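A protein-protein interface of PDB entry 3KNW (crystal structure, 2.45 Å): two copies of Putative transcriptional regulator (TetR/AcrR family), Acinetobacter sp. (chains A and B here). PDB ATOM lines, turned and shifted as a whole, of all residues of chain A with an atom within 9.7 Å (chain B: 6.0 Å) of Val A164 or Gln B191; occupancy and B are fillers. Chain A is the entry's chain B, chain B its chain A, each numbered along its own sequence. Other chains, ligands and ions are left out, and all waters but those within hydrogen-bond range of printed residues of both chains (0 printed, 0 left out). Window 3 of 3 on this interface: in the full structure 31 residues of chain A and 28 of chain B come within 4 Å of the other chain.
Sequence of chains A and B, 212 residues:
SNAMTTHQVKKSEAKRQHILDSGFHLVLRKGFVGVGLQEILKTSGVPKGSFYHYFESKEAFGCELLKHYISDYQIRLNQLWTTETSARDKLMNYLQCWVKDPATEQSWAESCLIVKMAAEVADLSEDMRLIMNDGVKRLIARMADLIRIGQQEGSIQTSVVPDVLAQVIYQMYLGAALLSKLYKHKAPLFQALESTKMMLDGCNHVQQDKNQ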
ATOM      1  N   ILE A 140      28.766 -21.374  -8.374  1.00  0.00           N
ATOM      2  CA  ILE A 140      27.901 -22.005  -7.365  1.00  0.00           C
ATOM      3  C   ILE A 140      28.695 -23.104  -6.668  1.00  0.00           C
ATOM      4  O   ILE A 140      28.659 -23.249  -5.441  1.00  0.00           O
ATOM      5  CB  ILE A 140      26.603 -22.560  -7.977  1.00  0.00           C
ATOM      6  CG1 ILE A 140      25.763 -21.404  -8.489  1.00  0.00           C
ATOM      7  CG2 ILE A 140      25.841 -23.426  -6.952  1.00  0.00           C
ATOM      8  CD1 ILE A 140      24.554 -21.769  -9.353  1.00  0.00           C
ATOM      9  N   ALA A 141      29.426 -23.859  -7.480  1.00  0.00           N
ATOM     10  CA  ALA A 141      30.296 -24.961  -7.032  1.00  0.00           C
ATOM     11  C   ALA A 141      31.303 -24.502  -6.002  1.00  0.00           C
ATOM     12  O   ALA A 141      31.484 -25.173  -4.976  1.00  0.00           O
ATOM     13  CB  ALA A 141      31.020 -25.624  -8.248  1.00  0.00           C
ATOM     14  N   MET A 143      31.106 -21.593  -4.128  1.00  0.00           N
ATOM     15  CA  MET A 143      30.343 -21.233  -2.942  1.00  0.00           C
ATOM     16  C   MET A 143      30.079 -22.528  -2.130  1.00  0.00           C
ATOM     17  O   MET A 143      30.293 -22.549  -0.939  1.00  0.00           O
ATOM     18  CB  MET A 143      29.042 -20.500  -3.306  1.00  0.00           C
ATOM     19  CG  MET A 143      29.188 -19.131  -4.010  1.00  0.00           C
ATOM     20  SD  MET A 143      27.482 -18.417  -4.635  1.00  0.00           S
ATOM     21  CE  MET A 143      26.705 -18.672  -2.900  1.00  0.00           C
ATOM     22  N   ALA A 144      29.644 -23.616  -2.775  1.00  0.00           N
ATOM     23  CA  ALA A 144      29.365 -24.897  -2.048  1.00  0.00           C
ATOM     24  C   ALA A 144      30.594 -25.490  -1.320  1.00  0.00           C
ATOM     25  O   ALA A 144      30.486 -25.951  -0.171  1.00  0.00           O
ATOM     26  CB  ALA A 144      28.775 -25.941  -2.989  1.00  0.00           C
ATOM     27  N   ASP A 145      31.751 -25.457  -1.982  1.00  0.00           N
ATOM     28  CA  ASP A 145      32.975 -25.983  -1.401  1.00  0.00           C
ATOM     29  C   ASP A 145      33.265 -25.203  -0.122  1.00  0.00           C
ATOM     30  O   ASP A 145      33.751 -25.733   0.877  1.00  0.00           O
ATOM     31  CB  ASP A 145      34.159 -25.895  -2.403  1.00  0.00           C
ATOM     32  CG  ASP A 145      34.032 -26.894  -3.596  1.00  0.00           C
ATOM     33  OD1 ASP A 145      33.244 -27.884  -3.492  1.00  0.00           O
ATOM     34  OD2 ASP A 145      34.718 -26.689  -4.648  1.00  0.00           O
ATOM     35  N   ILE A 147      30.890 -23.682   1.659  1.00  0.00           N
ATOM     36  CA  ILE A 147      29.941 -24.029   2.705  1.00  0.00           C
ATOM     37  C   ILE A 147      30.375 -25.289   3.424  1.00  0.00           C
ATOM     38  O   ILE A 147      30.229 -25.371   4.602  1.00  0.00           O
ATOM     39  CB  ILE A 147      28.537 -24.079   2.200  1.00  0.00           C
ATOM     40  CG1 ILE A 147      28.071 -22.654   1.853  1.00  0.00           C
ATOM     41  CG2 ILE A 147      27.636 -24.613   3.214  1.00  0.00           C
ATOM     42  CD1 ILE A 147      26.821 -22.617   0.878  1.00  0.00           C
ATOM     43  N   ARG A 148      30.985 -26.221   2.707  1.00  0.00           N
ATOM     44  CA  ARG A 148      31.380 -27.541   3.208  1.00  0.00           C
ATOM     45  C   ARG A 148      32.539 -27.435   4.208  1.00  0.00           C
ATOM     46  O   ARG A 148      32.445 -27.906   5.325  1.00  0.00           O
ATOM     47  CB  ARG A 148      31.795 -28.424   2.024  1.00  0.00           C
ATOM     48  CG  ARG A 148      32.233 -29.856   2.400  1.00  0.00           C
ATOM     49  CD  ARG A 148      32.641 -30.670   1.174  1.00  0.00           C
ATOM     50  NE  ARG A 148      31.633 -30.640   0.097  1.00  0.00           N
ATOM     51  CZ  ARG A 148      31.772 -30.018  -1.087  1.00  0.00           C
ATOM     52  NH1 ARG A 148      32.897 -29.356  -1.404  1.00  0.00           N
ATOM     53  NH2 ARG A 148      30.777 -30.062  -1.980  1.00  0.00           N
ATOM     54  N   GLN A 151      31.039 -25.773   7.324  1.00  0.00           N
ATOM     55  CA  GLN A 151      30.419 -26.816   8.187  1.00  0.00           C
ATOM     56  C   GLN A 151      31.449 -27.744   8.846  1.00  0.00           C
ATOM     57  O   GLN A 151      31.270 -28.137   9.985  1.00  0.00           O
ATOM     58  CB  GLN A 151      29.423 -27.664   7.393  1.00  0.00           C
ATOM     59  CG  GLN A 151      28.174 -26.903   6.959  1.00  0.00           C
ATOM     60  CD  GLN A 151      27.378 -27.580   5.823  1.00  0.00           C
ATOM     61  OE1 GLN A 151      27.956 -28.095   4.850  1.00  0.00           O
ATOM     62  NE2 GLN A 151      26.040 -27.531   5.927  1.00  0.00           N
ATOM     63  N   THR A 158      24.619 -24.831   9.937  1.00  0.00           N
ATOM     64  CA  THR A 158      23.462 -25.481   9.348  1.00  0.00           C
ATOM     65  C   THR A 158      23.873 -26.876   8.898  1.00  0.00           C
ATOM     66  O   THR A 158      25.059 -27.112   8.627  1.00  0.00           O
ATOM     67  CB  THR A 158      22.878 -24.738   8.127  1.00  0.00           C
ATOM     68  OG1 THR A 158      21.819 -25.521   7.560  1.00  0.00           O
ATOM     69  CG2 THR A 158      23.934 -24.481   7.044  1.00  0.00           C
ATOM     70  N   SER A 159      22.878 -27.769   8.816  1.00  0.00           N
ATOM     71  CA  SER A 159      23.066 -29.125   8.380  1.00  0.00           C
ATOM     72  C   SER A 159      22.757 -29.296   6.897  1.00  0.00           C
ATOM     73  O   SER A 159      23.206 -30.276   6.321  1.00  0.00           O
ATOM     74  CB  SER A 159      22.160 -30.067   9.184  1.00  0.00           C
ATOM     75  OG  SER A 159      20.787 -29.899   8.810  1.00  0.00           O
ATOM     76  N   VAL A 160      21.993 -28.379   6.285  1.00  0.00           N
ATOM     77  CA  VAL A 160      21.660 -28.469   4.844  1.00  0.00           C
ATOM     78  C   VAL A 160      22.838 -28.686   3.903  1.00  0.00           C
ATOM     79  O   VAL A 160      23.875 -28.041   4.041  1.00  0.00           O
ATOM     80  CB  VAL A 160      21.031 -27.197   4.307  1.00  0.00           C
ATOM     81  CG1 VAL A 160      20.988 -27.277   2.782  1.00  0.00           C
ATOM     82  CG2 VAL A 160      19.667 -26.995   4.877  1.00  0.00           C
ATOM     83  N   VAL A 161      22.654 -29.545   2.908  1.00  0.00           N
ATOM     84  CA  VAL A 161      23.757 -29.938   2.045  1.00  0.00           C
ATOM     85  C   VAL A 161      24.297 -28.730   1.262  1.00  0.00           C
ATOM     86  O   VAL A 161      23.540 -27.928   0.732  1.00  0.00           O
ATOM     87  CB  VAL A 161      23.391 -31.124   1.087  1.00  0.00           C
ATOM     88  CG1 VAL A 161      24.498 -31.317   0.039  1.00  0.00           C
ATOM     89  CG2 VAL A 161      23.164 -32.433   1.881  1.00  0.00           C
ATOM     90  N   PRO A 162      25.620 -28.600   1.214  1.00  0.00           N
ATOM     91  CA  PRO A 162      26.273 -27.538   0.498  1.00  0.00           C
ATOM     92  C   PRO A 162      25.722 -27.278  -0.863  1.00  0.00           C
ATOM     93  O   PRO A 162      25.394 -26.153  -1.139  1.00  0.00           O
ATOM     94  CB  PRO A 162      27.725 -28.026   0.397  1.00  0.00           C
ATOM     95  CG  PRO A 162      27.919 -28.880   1.609  1.00  0.00           C
ATOM     96  CD  PRO A 162      26.593 -29.458   1.937  1.00  0.00           C
ATOM     97  N   ASP A 163      25.616 -28.266  -1.732  1.00  0.00           N
ATOM     98  CA  ASP A 163      25.260 -27.957  -3.112  1.00  0.00           C
ATOM     99  C   ASP A 163      23.882 -27.340  -3.189  1.00  0.00           C
ATOM    100  O   ASP A 163      23.582 -26.576  -4.140  1.00  0.00           O
ATOM    101  CB  ASP A 163      25.428 -29.165  -4.053  1.00  0.00           C
ATOM    102  CG  ASP A 163      26.903 -29.621  -4.146  1.00  0.00           C
ATOM    103  OD1 ASP A 163      27.556 -29.756  -3.051  1.00  0.00           O
ATOM    104  OD2 ASP A 163      27.422 -29.819  -5.278  1.00  0.00           O
ATOM    105  N   VAL A 164      23.060 -27.645  -2.177  1.00  0.00           N
ATOM    106  CA  VAL A 164      21.716 -27.089  -2.072  1.00  0.00           C
ATOM    107  C   VAL A 164      21.788 -25.704  -1.513  1.00  0.00           C
ATOM    108  O   VAL A 164      21.194 -24.801  -2.059  1.00  0.00           O
ATOM    109  CB  VAL A 164      20.763 -27.908  -1.155  1.00  0.00           C
ATOM    110  CG1 VAL A 164      19.444 -27.150  -0.976  1.00  0.00           C
ATOM    111  CG2 VAL A 164      20.505 -29.300  -1.735  1.00  0.00           C
ATOM    112  N   LEU A 165      22.503 -25.506  -0.408  1.00  0.00           N
ATOM    113  CA  LEU A 165      22.541 -24.171   0.170  1.00  0.00           C
ATOM    114  C   LEU A 165      23.177 -23.141  -0.796  1.00  0.00           C
ATOM    115  O   LEU A 165      22.604 -22.083  -1.070  1.00  0.00           O
ATOM    116  CB  LEU A 165      23.249 -24.226   1.505  1.00  0.00           C
ATOM    117  CG  LEU A 165      23.073 -23.079   2.480  1.00  0.00           C
ATOM    118  CD1 LEU A 165      21.578 -22.672   2.622  1.00  0.00           C
ATOM    119  CD2 LEU A 165      23.655 -23.587   3.771  1.00  0.00           C
ATOM    120  N   ALA A 166      24.324 -23.483  -1.365  1.00  0.00           N
ATOM    121  CA  ALA A 166      24.924 -22.646  -2.399  1.00  0.00           C
ATOM    122  C   ALA A 166      23.897 -22.092  -3.380  1.00  0.00           C
ATOM    123  O   ALA A 166      23.893 -20.919  -3.696  1.00  0.00           O
ATOM    124  CB  ALA A 166      26.026 -23.413  -3.143  1.00  0.00           C
ATOM    125  N   GLN A 167      23.035 -22.949  -3.862  1.00  0.00           N
ATOM    126  CA  GLN A 167      22.032 -22.597  -4.884  1.00  0.00           C
ATOM    127  C   GLN A 167      20.983 -21.692  -4.305  1.00  0.00           C
ATOM    128  O   GLN A 167      20.664 -20.665  -4.909  1.00  0.00           O
ATOM    129  CB  GLN A 167      21.326 -23.870  -5.412  1.00  0.00           C
ATOM    130  CG  GLN A 167      22.069 -24.615  -6.583  1.00  0.00           C
ATOM    131  CD  GLN A 167      21.442 -25.947  -6.881  1.00  0.00           C
ATOM    132  OE1 GLN A 167      20.584 -26.045  -7.754  1.00  0.00           O
ATOM    133  NE2 GLN A 167      21.819 -26.978  -6.113  1.00  0.00           N
ATOM    134  N   VAL A 168      20.400 -22.064  -3.166  1.00  0.00           N
ATOM    135  CA  VAL A 168      19.480 -21.164  -2.528  1.00  0.00           C
ATOM    136  C   VAL A 168      20.093 -19.746  -2.317  1.00  0.00           C
ATOM    137  O   VAL A 168      19.459 -18.715  -2.625  1.00  0.00           O
ATOM    138  CB  VAL A 168      19.079 -21.649  -1.154  1.00  0.00           C
ATOM    139  CG1 VAL A 168      18.388 -20.517  -0.391  1.00  0.00           C
ATOM    140  CG2 VAL A 168      18.206 -22.927  -1.253  1.00  0.00           C
ATOM    141  N   ILE A 169      21.306 -19.694  -1.759  1.00  0.00           N
ATOM    142  CA  ILE A 169      21.896 -18.396  -1.523  1.00  0.00           C
ATOM    143  C   ILE A 169      22.023 -17.696  -2.848  1.00  0.00           C
ATOM    144  O   ILE A 169      21.628 -16.511  -2.952  1.00  0.00           O
ATOM    145  CB  ILE A 169      23.207 -18.437  -0.882  1.00  0.00           C
ATOM    146  CG1 ILE A 169      23.041 -18.878   0.572  1.00  0.00           C
ATOM    147  CG2 ILE A 169      23.866 -17.063  -0.935  1.00  0.00           C
ATOM    148  CD1 ILE A 169      24.385 -19.184   1.251  1.00  0.00           C
ATOM    149  N   TYR A 170      22.480 -18.416  -3.888  1.00  0.00           N
ATOM    150  CA  TYR A 170      22.788 -17.668  -5.110  1.00  0.00           C
ATOM    151  C   TYR A 170      21.514 -17.179  -5.789  1.00  0.00           C
ATOM    152  O   TYR A 170      21.439 -16.052  -6.253  1.00  0.00           O
ATOM    153  CB  TYR A 170      23.664 -18.478  -6.050  1.00  0.00           C
ATOM    154  CG  TYR A 170      24.166 -17.673  -7.237  1.00  0.00           C
ATOM    155  CD1 TYR A 170      25.184 -16.741  -7.109  1.00  0.00           C
ATOM    156  CD2 TYR A 170      23.604 -17.844  -8.491  1.00  0.00           C
ATOM    157  CE1 TYR A 170      25.623 -15.968  -8.215  1.00  0.00           C
ATOM    158  CE2 TYR A 170      24.031 -17.086  -9.589  1.00  0.00           C
ATOM    159  CZ  TYR A 170      25.040 -16.152  -9.461  1.00  0.00           C
ATOM    160  OH  TYR A 170      25.427 -15.415 -10.610  1.00  0.00           O
ATOM    161  N   GLN A 171      20.505 -18.020  -5.846  1.00  0.00           N
ATOM    162  CA  GLN A 171      19.282 -17.635  -6.416  1.00  0.00           C
ATOM    163  C   GLN A 171      18.676 -16.470  -5.651  1.00  0.00           C
ATOM    164  O   GLN A 171      18.137 -15.551  -6.278  1.00  0.00           O
ATOM    165  CB  GLN A 171      18.292 -18.803  -6.459  1.00  0.00           C
ATOM    166  CG  GLN A 171      18.620 -19.884  -7.502  1.00  0.00           C
ATOM    167  CD  GLN A 171      17.766 -21.130  -7.318  1.00  0.00           C
ATOM    168  OE1 GLN A 171      16.859 -21.162  -6.512  1.00  0.00           O
ATOM    169  NE2 GLN A 171      18.058 -22.140  -8.066  1.00  0.00           N
ATOM    170  N   MET A 172      18.748 -16.505  -4.317  1.00  0.00           N
ATOM    171  CA  MET A 172      18.175 -15.421  -3.475  1.00  0.00           C
ATOM    172  C   MET A 172      18.804 -14.111  -3.874  1.00  0.00           C
ATOM    173  O   MET A 172      18.101 -13.103  -4.120  1.00  0.00           O
ATOM    174  CB  MET A 172      18.408 -15.689  -1.977  1.00  0.00           C
ATOM    175  CG  MET A 172      17.637 -14.756  -1.025  1.00  0.00           C
ATOM    176  SD  MET A 172      17.709 -15.260   0.763  1.00  0.00           S
ATOM    177  CE  MET A 172      19.581 -15.325   0.894  1.00  0.00           C
ATOM    178  N   MET A 199      20.402 -18.497   7.692  1.00  0.00           N
ATOM    179  CA  MET A 199      20.507 -19.797   6.997  1.00  0.00           C
ATOM    180  C   MET A 199      21.843 -20.440   7.292  1.00  0.00           C
ATOM    181  O   MET A 199      21.941 -21.669   7.339  1.00  0.00           O
ATOM    182  CB  MET A 199      20.347 -19.685   5.475  1.00  0.00           C
ATOM    183  CG  MET A 199      18.990 -19.252   5.048  1.00  0.00           C
ATOM    184  SD  MET A 199      18.828 -18.900   3.171  1.00  0.00           S
ATOM    185  CE  MET A 199      19.784 -17.306   3.007  1.00  0.00           C
ATOM    186  N   MET B 172      14.221 -16.018  -4.206  1.00  0.00           N
ATOM    187  CA  MET B 172      14.776 -17.283  -4.695  1.00  0.00           C
ATOM    188  C   MET B 172      14.092 -17.757  -5.910  1.00  0.00           C
ATOM    189  O   MET B 172      14.759 -18.228  -6.831  1.00  0.00           O
ATOM    190  CB  MET B 172      14.718 -18.360  -3.631  1.00  0.00           C
ATOM    191  CG  MET B 172      15.129 -19.788  -4.089  1.00  0.00           C
ATOM    192  SD  MET B 172      14.960 -20.954  -2.540  1.00  0.00           S
ATOM    193  CE  MET B 172      13.097 -21.249  -2.556  1.00  0.00           C
ATOM    194  N   LYS B 186      14.584 -26.022 -16.467  1.00  0.00           N
ATOM    195  CA  LYS B 186      14.079 -25.510 -15.238  1.00  0.00           C
ATOM    196  C   LYS B 186      14.631 -26.198 -14.032  1.00  0.00           C
ATOM    197  O   LYS B 186      14.094 -26.091 -12.915  1.00  0.00           O
ATOM    198  CB  LYS B 186      12.553 -25.541 -15.257  1.00  0.00           C
ATOM    199  CG  LYS B 186      11.980 -24.660 -16.340  1.00  0.00           C
ATOM    200  CD  LYS B 186      10.519 -24.928 -16.491  1.00  0.00           C
ATOM    201  CE  LYS B 186       9.815 -24.007 -17.451  1.00  0.00           C
ATOM    202  NZ  LYS B 186       8.331 -24.332 -17.469  1.00  0.00           N
ATOM    203  N   ALA B 187      15.750 -26.847 -14.196  1.00  0.00           N
ATOM    204  CA  ALA B 187      16.408 -27.487 -13.030  1.00  0.00           C
ATOM    205  C   ALA B 187      16.447 -26.507 -11.835  1.00  0.00           C
ATOM    206  O   ALA B 187      16.054 -26.855 -10.720  1.00  0.00           O
ATOM    207  CB  ALA B 187      17.859 -28.024 -13.403  1.00  0.00           C
ATOM    208  N   PRO B 188      16.871 -25.270 -12.043  1.00  0.00           N
ATOM    209  CA  PRO B 188      16.947 -24.371 -10.838  1.00  0.00           C
ATOM    210  C   PRO B 188      15.637 -24.136 -10.116  1.00  0.00           C
ATOM    211  O   PRO B 188      15.630 -23.992  -8.889  1.00  0.00           O
ATOM    212  CB  PRO B 188      17.512 -23.075 -11.422  1.00  0.00           C
ATOM    213  CG  PRO B 188      18.318 -23.493 -12.579  1.00  0.00           C
ATOM    214  CD  PRO B 188      17.638 -24.723 -13.183  1.00  0.00           C
ATOM    215  N   LEU B 189      14.546 -24.100 -10.872  1.00  0.00           N
ATOM    216  CA  LEU B 189      13.173 -23.894 -10.360  1.00  0.00           C
ATOM    217  C   LEU B 189      12.685 -25.149  -9.683  1.00  0.00           C
ATOM    218  O   LEU B 189      12.097 -25.081  -8.630  1.00  0.00           O
ATOM    219  CB  LEU B 189      12.171 -23.560 -11.484  1.00  0.00           C
ATOM    220  CG  LEU B 189      12.148 -22.115 -11.922  1.00  0.00           C
ATOM    221  CD1 LEU B 189      11.565 -21.834 -13.325  1.00  0.00           C
ATOM    222  CD2 LEU B 189      11.411 -21.288 -10.875  1.00  0.00           C
ATOM    223  N   PHE B 190      13.005 -26.305 -10.249  1.00  0.00           N
ATOM    224  CA  PHE B 190      12.763 -27.542  -9.556  1.00  0.00           C
ATOM    225  C   PHE B 190      13.445 -27.614  -8.207  1.00  0.00           C
ATOM    226  O   PHE B 190      12.864 -28.160  -7.239  1.00  0.00           O
ATOM    227  CB  PHE B 190      13.158 -28.757 -10.402  1.00  0.00           C
ATOM    228  CG  PHE B 190      12.496 -28.809 -11.792  1.00  0.00           C
ATOM    229  CD1 PHE B 190      11.228 -28.301 -12.011  1.00  0.00           C
ATOM    230  CD2 PHE B 190      13.142 -29.439 -12.846  1.00  0.00           C
ATOM    231  CE1 PHE B 190      10.648 -28.370 -13.235  1.00  0.00           C
ATOM    232  CE2 PHE B 190      12.573 -29.503 -14.097  1.00  0.00           C
ATOM    233  CZ  PHE B 190      11.327 -28.991 -14.310  1.00  0.00           C
ATOM    234  N   GLN B 191      14.663 -27.100  -8.101  1.00  0.00           N
ATOM    235  CA  GLN B 191      15.358 -27.183  -6.797  1.00  0.00           C
ATOM    236  C   GLN B 191      14.678 -26.192  -5.812  1.00  0.00           C
ATOM    237  O   GLN B 191      14.375 -26.580  -4.700  1.00  0.00           O
ATOM    238  CB  GLN B 191      16.869 -26.937  -6.930  1.00  0.00           C
ATOM    239  CG  GLN B 191      17.687 -26.993  -5.584  1.00  0.00           C
ATOM    240  CD  GLN B 191      17.332 -28.212  -4.706  1.00  0.00           C
ATOM    241  OE1 GLN B 191      17.480 -29.389  -5.117  1.00  0.00           O
ATOM    242  NE2 GLN B 191      16.813 -27.929  -3.514  1.00  0.00           N
ATOM    243  N   ALA B 192      14.379 -24.961  -6.241  1.00  0.00           N
ATOM    244  CA  ALA B 192      13.618 -23.992  -5.445  1.00  0.00           C
ATOM    245  C   ALA B 192      12.364 -24.625  -4.807  1.00  0.00           C
ATOM    246  O   ALA B 192      12.061 -24.384  -3.629  1.00  0.00           O
ATOM    247  CB  ALA B 192      13.143 -22.836  -6.345  1.00  0.00           C
ATOM    248  N   LEU B 193      11.619 -25.381  -5.624  1.00  0.00           N
ATOM    249  CA  LEU B 193      10.473 -26.158  -5.135  1.00  0.00           C
ATOM    250  C   LEU B 193      10.839 -27.058  -3.972  1.00  0.00           C
ATOM    251  O   LEU B 193      10.198 -27.052  -2.944  1.00  0.00           O
ATOM    252  CB  LEU B 193       9.825 -26.996  -6.256  1.00  0.00           C
ATOM    253  CG  LEU B 193       8.806 -26.223  -7.125  1.00  0.00           C
ATOM    254  CD1 LEU B 193       8.331 -27.055  -8.335  1.00  0.00           C
ATOM    255  CD2 LEU B 193       7.582 -25.764  -6.269  1.00  0.00           C
ATOM    256  N   GLU B 194      11.907 -27.808  -4.133  1.00  0.00           N
ATOM    257  CA  GLU B 194      12.281 -28.789  -3.110  1.00  0.00           C
ATOM    258  C   GLU B 194      12.770 -28.038  -1.876  1.00  0.00           C
ATOM    259  O   GLU B 194      12.454 -28.383  -0.770  1.00  0.00           O
ATOM    260  CB  GLU B 194      13.295 -29.824  -3.660  1.00  0.00           C
ATOM    261  CG  GLU B 194      13.414 -31.088  -2.794  1.00  0.00           C
ATOM    262  CD  GLU B 194      12.075 -31.872  -2.596  1.00  0.00           C
ATOM    263  OE1 GLU B 194      11.941 -32.610  -1.573  1.00  0.00           O
ATOM    264  OE2 GLU B 194      11.172 -31.761  -3.478  1.00  0.00           O
ATOM    265  N   SER B 195      13.469 -26.938  -2.090  1.00  0.00           N
ATOM    266  CA  SER B 195      13.916 -26.088  -1.018  1.00  0.00           C
ATOM    267  C   SER B 195      12.833 -25.333  -0.237  1.00  0.00           C
ATOM    268  O   SER B 195      12.964 -25.193   0.978  1.00  0.00           O
ATOM    269  CB  SER B 195      14.966 -25.125  -1.569  1.00  0.00           C
ATOM    270  OG  SER B 195      16.217 -25.801  -1.487  1.00  0.00           O
ATOM    271  N   THR B 196      11.793 -24.856  -0.914  1.00  0.00           N
ATOM    272  CA  THR B 196      10.691 -24.209  -0.251  1.00  0.00           C
ATOM    273  C   THR B 196      10.039 -25.131   0.838  1.00  0.00           C
ATOM    274  O   THR B 196       9.464 -24.632   1.819  1.00  0.00           O
ATOM    275  CB  THR B 196       9.591 -23.781  -1.263  1.00  0.00           C
ATOM    276  OG1 THR B 196      10.165 -22.993  -2.315  1.00  0.00           O
ATOM    277  CG2 THR B 196       8.467 -22.978  -0.559  1.00  0.00           C
ATOM    278  N   MET B 198      11.760 -27.625   2.899  1.00  0.00           N
ATOM    279  CA  MET B 198      12.618 -27.364   4.067  1.00  0.00           C
ATOM    280  C   MET B 198      12.242 -26.055   4.784  1.00  0.00           C
ATOM    281  O   MET B 198      12.014 -26.022   5.981  1.00  0.00           O
ATOM    282  CB  MET B 198      14.109 -27.254   3.654  1.00  0.00           C
ATOM    283  CG  MET B 198      14.601 -28.271   2.587  1.00  0.00           C
ATOM    284  SD  MET B 198      16.575 -28.584   2.525  1.00  0.00           S
ATOM    285  CE  MET B 198      16.558 -30.537   2.308  1.00  0.00           C
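The backbone carbonyl oxygen of Pro B188 sits at hydrogen-bond distance from the side-chain amide nitrogen of Gln A171 (3.2 Å).
The side-chain amide nitrogen (NE2) of Gln B191 sits at hydrogen-bond distance from the side-chain hydroxyl (OG) of Ser B195, 3.0 Å away. O of Asp A163 lies within hydrogen-bond range of NE2 of Gln A167.
Among the printed residues, merely in contact across the chains: Gln A171 with Met B172 (3.3 Å), Val A168 with Ser B195 (3.5 Å), Val A164 with Ser B195 (3.5 Å), Val A164 with Gln B191 (3.7 Å) and Gln A167 with Gln B191 (3.7 Å).
Of the printed residues of chain B, Val A164 touches Gln B191 and Ser B195. Printed residues of chain B within 4 Å of Val A168: Ser B195 (3.5 Å). Gln B191 touches just these residues of chain A: Val A164 (3.7 Å) and Gln A167 (3.7 Å). Leu B193 touches none of the printed residues of chain A. Printed residues of chain A within 4 Å of Ser B195: Val A164 and Val A168. The nearest residue of chain B that does not touch Val A164 is Met B198 (4.7 Å). The nearest residue of chain A that does not touch Gln B191 is Gln A171 (5.1 Å). The nearest printed residue of chain A that does not touch Met B172 is Val A168 (4.01 Å).
Printed residues of chain B that touch a printed residue of chain A: Met B172, Pro B188, Gln B191 and Ser B195. Of the 24 printed residues of chain A, 4 touch a printed residue of chain B. Printed residues of chain A that touch a printed residue of chain B: Val A164, Gln A167, Val A168 and Gln A171. Hydrophobic or aromatic side chains of chain A that line the printed part of chain B: Val A164 and Val A168. Among the printed residues, no Asp or Glu carboxylate lies within 4 Å of a Lys or Arg side-chain nitrogen of the other chain.
Position printed for both chains: 172. Of the 6 pairs that touch across the chains among the printed residues, none has its exchanged pair printed and touching as well.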
